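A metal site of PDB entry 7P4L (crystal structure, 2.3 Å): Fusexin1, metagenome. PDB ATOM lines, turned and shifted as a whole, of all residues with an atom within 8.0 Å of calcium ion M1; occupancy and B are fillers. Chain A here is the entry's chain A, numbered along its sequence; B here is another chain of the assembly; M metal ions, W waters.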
ATOM      1  N   TYR A  68      18.392   3.491  14.149  1.00  0.00           N
ATOM      2  CA  TYR A  68      16.962   3.629  14.378  1.00  0.00           C
ATOM      3  C   TYR A  68      16.479   2.611  15.398  1.00  0.00           C
ATOM      4  O   TYR A  68      17.165   1.631  15.720  1.00  0.00           O
ATOM      5  CB  TYR A  68      16.190   3.451  13.070  1.00  0.00           C
ATOM      6  CG  TYR A  68      16.310   4.639  12.149  1.00  0.00           C
ATOM      7  CD1 TYR A  68      17.359   4.723  11.239  1.00  0.00           C
ATOM      8  CD2 TYR A  68      15.379   5.666  12.188  1.00  0.00           C
ATOM      9  CE1 TYR A  68      17.473   5.810  10.391  1.00  0.00           C
ATOM     10  CE2 TYR A  68      15.492   6.756  11.348  1.00  0.00           C
ATOM     11  CZ  TYR A  68      16.546   6.823  10.448  1.00  0.00           C
ATOM     12  OH  TYR A  68      16.673   7.899   9.617  1.00  0.00           O
ATOM     13  N   SER A  69      15.298   2.871  15.945  1.00  0.00           N
ATOM     14  CA  SER A  69      14.580   1.913  16.770  1.00  0.00           C
ATOM     15  C   SER A  69      13.094   2.035  16.442  1.00  0.00           C
ATOM     16  O   SER A  69      12.675   2.904  15.671  1.00  0.00           O
ATOM     17  CB  SER A  69      14.860   2.158  18.262  1.00  0.00           C
ATOM     18  OG  SER A  69      14.418   3.435  18.686  1.00  0.00           O
ATOM     19  N   THR A  70      12.298   1.159  17.040  1.00  0.00           N
ATOM     20  CA  THR A  70      10.861   1.123  16.784  1.00  0.00           C
ATOM     21  C   THR A  70      10.098   1.102  18.100  1.00  0.00           C
ATOM     22  O   THR A  70      10.667   0.874  19.169  1.00  0.00           O
ATOM     23  CB  THR A  70      10.476  -0.102  15.942  1.00  0.00           C
ATOM     24  OG1 THR A  70      10.733  -1.301  16.686  1.00  0.00           O
ATOM     25  CG2 THR A  70      11.265  -0.148  14.639  1.00  0.00           C
ATOM     26  N   SER A  71       8.808   1.390  18.020  1.00  0.00           N
ATOM     27  CA  SER A  71       7.943   1.395  19.191  1.00  0.00           C
ATOM     28  C   SER A  71       6.569   0.841  18.819  1.00  0.00           C
ATOM     29  O   SER A  71       5.933   1.333  17.893  1.00  0.00           O
ATOM     30  CB  SER A  71       7.794   2.804  19.775  1.00  0.00           C
ATOM     31  OG  SER A  71       9.053   3.459  19.841  1.00  0.00           O
ATOM     32  N   THR A  72       6.141  -0.194  19.537  1.00  0.00           N
ATOM     33  CA  THR A  72       4.781  -0.684  19.414  1.00  0.00           C
ATOM     34  C   THR A  72       3.866   0.093  20.363  1.00  0.00           C
ATOM     35  O   THR A  72       4.305   0.894  21.186  1.00  0.00           O
ATOM     36  CB  THR A  72       4.712  -2.176  19.751  1.00  0.00           C
ATOM     37  OG1 THR A  72       5.163  -2.383  21.091  1.00  0.00           O
ATOM     38  CG2 THR A  72       5.544  -2.990  18.791  1.00  0.00           C
ATOM     39  N   ALA A 145       4.724  -1.001  14.220  1.00  0.00           N
ATOM     40  CA  ALA A 145       5.436  -0.242  15.232  1.00  0.00           C
ATOM     41  C   ALA A 145       5.837   1.108  14.645  1.00  0.00           C
ATOM     42  O   ALA A 145       6.122   1.218  13.458  1.00  0.00           O
ATOM     43  CB  ALA A 145       6.669  -0.986  15.727  1.00  0.00           C
ATOM     44  N   TYR A 146       5.857   2.130  15.492  1.00  0.00           N
ATOM     45  CA  TYR A 146       6.436   3.403  15.093  1.00  0.00           C
ATOM     46  C   TYR A 146       7.944   3.242  14.892  1.00  0.00           C
ATOM     47  O   TYR A 146       8.565   2.359  15.474  1.00  0.00           O
ATOM     48  CB  TYR A 146       6.196   4.473  16.152  1.00  0.00           C
ATOM     49  CG  TYR A 146       4.763   4.853  16.406  1.00  0.00           C
ATOM     50  CD1 TYR A 146       4.104   5.735  15.575  1.00  0.00           C
ATOM     51  CD2 TYR A 146       4.090   4.365  17.515  1.00  0.00           C
ATOM     52  CE1 TYR A 146       2.785   6.105  15.821  1.00  0.00           C
ATOM     53  CE2 TYR A 146       2.783   4.733  17.774  1.00  0.00           C
ATOM     54  CZ  TYR A 146       2.138   5.595  16.920  1.00  0.00           C
ATOM     55  OH  TYR A 146       0.842   5.957  17.183  1.00  0.00           O
ATOM     56  N   ILE A 147       8.508   4.115  14.064  1.00  0.00           N
ATOM     57  CA  ILE A 147       9.959   4.206  13.867  1.00  0.00           C
ATOM     58  C   ILE A 147      10.438   5.484  14.545  1.00  0.00           C
ATOM     59  O   ILE A 147       9.981   6.589  14.224  1.00  0.00           O
ATOM     60  CB  ILE A 147      10.333   4.193  12.379  1.00  0.00           C
ATOM     61  CG1 ILE A 147      10.001   2.821  11.783  1.00  0.00           C
ATOM     62  CG2 ILE A 147      11.834   4.516  12.183  1.00  0.00           C
ATOM     63  CD1 ILE A 147      10.270   2.687  10.314  1.00  0.00           C
ATOM     64  N   ASP A 148      11.383   5.346  15.475  1.00  0.00           N
ATOM     65  CA  ASP A 148      11.798   6.477  16.300  1.00  0.00           C
ATOM     66  C   ASP A 148      12.870   7.301  15.605  1.00  0.00           C
ATOM     67  O   ASP A 148      13.501   6.872  14.638  1.00  0.00           O
ATOM     68  CB  ASP A 148      12.325   5.985  17.655  1.00  0.00           C
ATOM     69  CG  ASP A 148      11.405   4.984  18.316  1.00  0.00           C
ATOM     70  OD1 ASP A 148      10.169   5.118  18.159  1.00  0.00           O
ATOM     71  OD2 ASP A 148      11.915   4.062  18.987  1.00  0.00           O
ATOM     72  N   ASN A 149      13.083   8.513  16.126  1.00  0.00           N
ATOM     73  CA  ASN A 149      14.160   9.344  15.641  1.00  0.00           C
ATOM     74  C   ASN A 149      15.497   8.650  15.895  1.00  0.00           C
ATOM     75  O   ASN A 149      15.706   8.065  16.955  1.00  0.00           O
ATOM     76  CB  ASN A 149      14.148  10.711  16.323  1.00  0.00           C
ATOM     77  CG  ASN A 149      13.001  11.576  15.842  1.00  0.00           C
ATOM     78  OD1 ASN A 149      12.497  11.377  14.746  1.00  0.00           O
ATOM     79  ND2 ASN A 149      12.576  12.524  16.667  1.00  0.00           N
ATOM     80  N   ARG B 207       3.818  12.156  16.498  1.00  0.00           N
ATOM     81  CA  ARG B 207       2.904  11.096  16.909  1.00  0.00           C
ATOM     82  C   ARG B 207       1.867  11.556  17.906  1.00  0.00           C
ATOM     83  O   ARG B 207       0.956  10.781  18.220  1.00  0.00           O
ATOM     84  CB  ARG B 207       3.658   9.959  17.606  1.00  0.00           C
ATOM     85  CG  ARG B 207       4.760   9.336  16.842  1.00  0.00           C
ATOM     86  CD  ARG B 207       5.433   8.315  17.733  1.00  0.00           C
ATOM     87  NE  ARG B 207       6.620   7.785  17.086  1.00  0.00           N
ATOM     88  CZ  ARG B 207       7.576   7.107  17.705  1.00  0.00           C
ATOM     89  NH1 ARG B 207       7.496   6.833  18.990  1.00  0.00           N
ATOM     90  NH2 ARG B 207       8.630   6.702  17.006  1.00  0.00           N
ATOM     91  N   SER B 275       2.911   5.482  27.489  1.00  0.00           N
ATOM     92  CA  SER B 275       4.344   5.695  27.622  1.00  0.00           C
ATOM     93  C   SER B 275       5.108   5.020  26.497  1.00  0.00           C
ATOM     94  O   SER B 275       6.160   5.520  26.075  1.00  0.00           O
ATOM     95  CB  SER B 275       4.829   5.160  28.960  1.00  0.00           C
ATOM     96  OG  SER B 275       6.215   5.404  29.108  1.00  0.00           O
ATOM     97  N   SER B 276       4.597   3.901  25.984  1.00  0.00           N
ATOM     98  CA  SER B 276       5.248   3.228  24.872  1.00  0.00           C
ATOM     99  C   SER B 276       5.169   4.066  23.593  1.00  0.00           C
ATOM    100  O   SER B 276       6.047   3.960  22.731  1.00  0.00           O
ATOM    101  CB  SER B 276       4.620   1.854  24.633  1.00  0.00           C
ATOM    102  OG  SER B 276       3.245   1.983  24.289  1.00  0.00           O
ATOM    103  N   THR B 277       4.135   4.889  23.468  1.00  0.00           N
ATOM    104  CA  THR B 277       3.983   5.697  22.255  1.00  0.00           C
ATOM    105  C   THR B 277       5.033   6.795  22.183  1.00  0.00           C
ATOM    106  O   THR B 277       5.572   7.069  21.103  1.00  0.00           O
ATOM    107  CB  THR B 277       2.565   6.282  22.206  1.00  0.00           C
ATOM    108  OG1 THR B 277       1.615   5.216  22.113  1.00  0.00           O
ATOM    109  CG2 THR B 277       2.406   7.208  21.001  1.00  0.00           C
ATOM    110  N   THR B 278       5.345   7.436  23.312  1.00  0.00           N
ATOM    111  CA  THR B 278       6.165   8.650  23.287  1.00  0.00           C
ATOM    112  C   THR B 278       7.011   8.767  24.553  1.00  0.00           C
ATOM    113  O   THR B 278       6.555   8.452  25.649  1.00  0.00           O
ATOM    114  CB  THR B 278       5.291   9.895  23.142  1.00  0.00           C
ATOM    115  OG1 THR B 278       6.091  11.073  23.189  1.00  0.00           O
ATOM    116  CG2 THR B 278       4.250   9.942  24.256  1.00  0.00           C
ATOM    117  N   ASP B 279       8.252   9.242  24.371  1.00  0.00           N
ATOM    118  CA  ASP B 279       9.093   9.586  25.523  1.00  0.00           C
ATOM    119  C   ASP B 279       8.563  10.804  26.272  1.00  0.00           C
ATOM    120  O   ASP B 279       8.988  11.039  27.411  1.00  0.00           O
ATOM    121  CB  ASP B 279      10.524   9.860  25.065  1.00  0.00           C
ATOM    122  CG  ASP B 279      11.234   8.612  24.570  1.00  0.00           C
ATOM    123  OD1 ASP B 279      10.927   7.512  25.062  1.00  0.00           O
ATOM    124  OD2 ASP B 279      12.120   8.741  23.692  1.00  0.00           O
ATOM    125  N   GLY B 342      10.243  -5.523  18.669  1.00  0.00           N
ATOM    126  CA  GLY B 342       9.409  -4.385  18.368  1.00  0.00           C
ATOM    127  C   GLY B 342       9.582  -3.208  19.307  1.00  0.00           C
ATOM    128  O   GLY B 342       9.142  -2.094  18.972  1.00  0.00           O
ATOM    129  N   ASP B 343      10.209  -3.408  20.467  1.00  0.00           N
ATOM    130  CA  ASP B 343      10.519  -2.337  21.403  1.00  0.00           C
ATOM    131  C   ASP B 343      11.931  -2.554  21.940  1.00  0.00           C
ATOM    132  O   ASP B 343      12.253  -3.680  22.350  1.00  0.00           O
ATOM    133  CB  ASP B 343       9.534  -2.300  22.582  1.00  0.00           C
ATOM    134  CG  ASP B 343       8.183  -1.743  22.205  1.00  0.00           C
ATOM    135  OD1 ASP B 343       8.093  -0.531  21.939  1.00  0.00           O
ATOM    136  OD2 ASP B 343       7.211  -2.520  22.190  1.00  0.00           O
ATOM    137  N   GLU B 344      12.740  -1.511  21.966  1.00  0.00           N
ATOM    138  CA  GLU B 344      14.085  -1.660  22.509  1.00  0.00           C
ATOM    139  C   GLU B 344      14.031  -1.881  24.016  1.00  0.00           C
ATOM    140  O   GLU B 344      13.228  -1.272  24.723  1.00  0.00           O
ATOM    141  CB  GLU B 344      14.932  -0.427  22.174  1.00  0.00           C
ATOM    142  CG  GLU B 344      14.572   0.852  22.917  1.00  0.00           C
ATOM    143  CD  GLU B 344      13.474   1.654  22.247  1.00  0.00           C
ATOM    144  OE1 GLU B 344      13.137   1.346  21.084  1.00  0.00           O
ATOM    145  OE2 GLU B 344      12.972   2.597  22.878  1.00  0.00           O
ATOM    146  N   GLY B 345      14.870  -2.788  24.494  1.00  0.00           N
ATOM    147  CA  GLY B 345      15.158  -2.904  25.909  1.00  0.00           C
ATOM    148  C   GLY B 345      16.383  -2.104  26.270  1.00  0.00           C
ATOM    149  O   GLY B 345      16.918  -1.325  25.475  1.00  0.00           O
ATOM    150  N   VAL B 375      21.253   0.386  19.669  1.00  0.00           N
ATOM    151  CA  VAL B 375      20.529   1.488  19.047  1.00  0.00           C
ATOM    152  C   VAL B 375      20.644   2.730  19.937  1.00  0.00           C
ATOM    153  O   VAL B 375      19.670   3.471  20.115  1.00  0.00           O
ATOM    154  CB  VAL B 375      19.062   1.129  18.760  1.00  0.00           C
ATOM    155  CG1 VAL B 375      19.012   0.071  17.682  1.00  0.00           C
ATOM    156  CG2 VAL B 375      18.349   0.655  20.004  1.00  0.00           C
ATOM    157  N   ASP B 394      20.076   1.546  25.025  1.00  0.00           N
ATOM    158  CA  ASP B 394      18.975   0.878  24.350  1.00  0.00           C
ATOM    159  C   ASP B 394      19.484  -0.225  23.430  1.00  0.00           C
ATOM    160  O   ASP B 394      20.400   0.007  22.625  1.00  0.00           O
ATOM    161  CB  ASP B 394      18.154   1.884  23.544  1.00  0.00           C
ATOM    162  CG  ASP B 394      17.413   2.875  24.423  1.00  0.00           C
ATOM    163  OD1 ASP B 394      17.240   2.594  25.626  1.00  0.00           O
ATOM    164  OD2 ASP B 394      16.999   3.939  23.891  1.00  0.00           O
HETATM  165 CA    CA M   1      11.153   2.773  20.904  1.00  0.00          CA
HETATM  166 CA    CA M   2      18.209   5.275  20.013  1.00  0.00          CA
HETATM  167  O   HOH W   1       9.997   1.590  22.478  1.00  0.00           O
HETATM  168  O   HOH W   2      11.291   4.489  22.961  1.00  0.00           O
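The backbone NH (N) of Asp 148 sits at hydrogen-bond distance from the backbone carbonyl oxygen (O) of Ser 69 (2.8 Å).
NH2 of Arg 207 of chain B lies within salt-bridge range of OD1 of Asp 148, at 2.5 Å.
OE1 of Glu 344 of chain B sits close to OG of Ser 69 (3.4 Å).
O of Ser 71 is in hydrogen-bond range of N of Tyr 146.
The backbone carbonyl oxygen (O) of Gly 342 of chain B is in hydrogen-bond range of the side-chain hydroxyl (OG1) of Thr 70, 2.9 Å away.
Four residues have an atom within 4 Å of calcium ion M1: Thr 70, Ser 71, Asp 148 and Glu 344 of chain B.
The nearest printed residue that does not touch calcium ion M1 is Ser 69 (4.002 Å).
Calcium ion M1 is bound by water W1, the side-chain carboxylate (OD2) of Asp 148, the side-chain carboxylate (OE1) of Glu 344 of chain B, the side-chain hydroxyl (OG) of Ser 71, the backbone carbonyl oxygen (O) of Thr 70, water W2 and the side-chain carboxylate (OE2) of Glu 344 of chain B.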
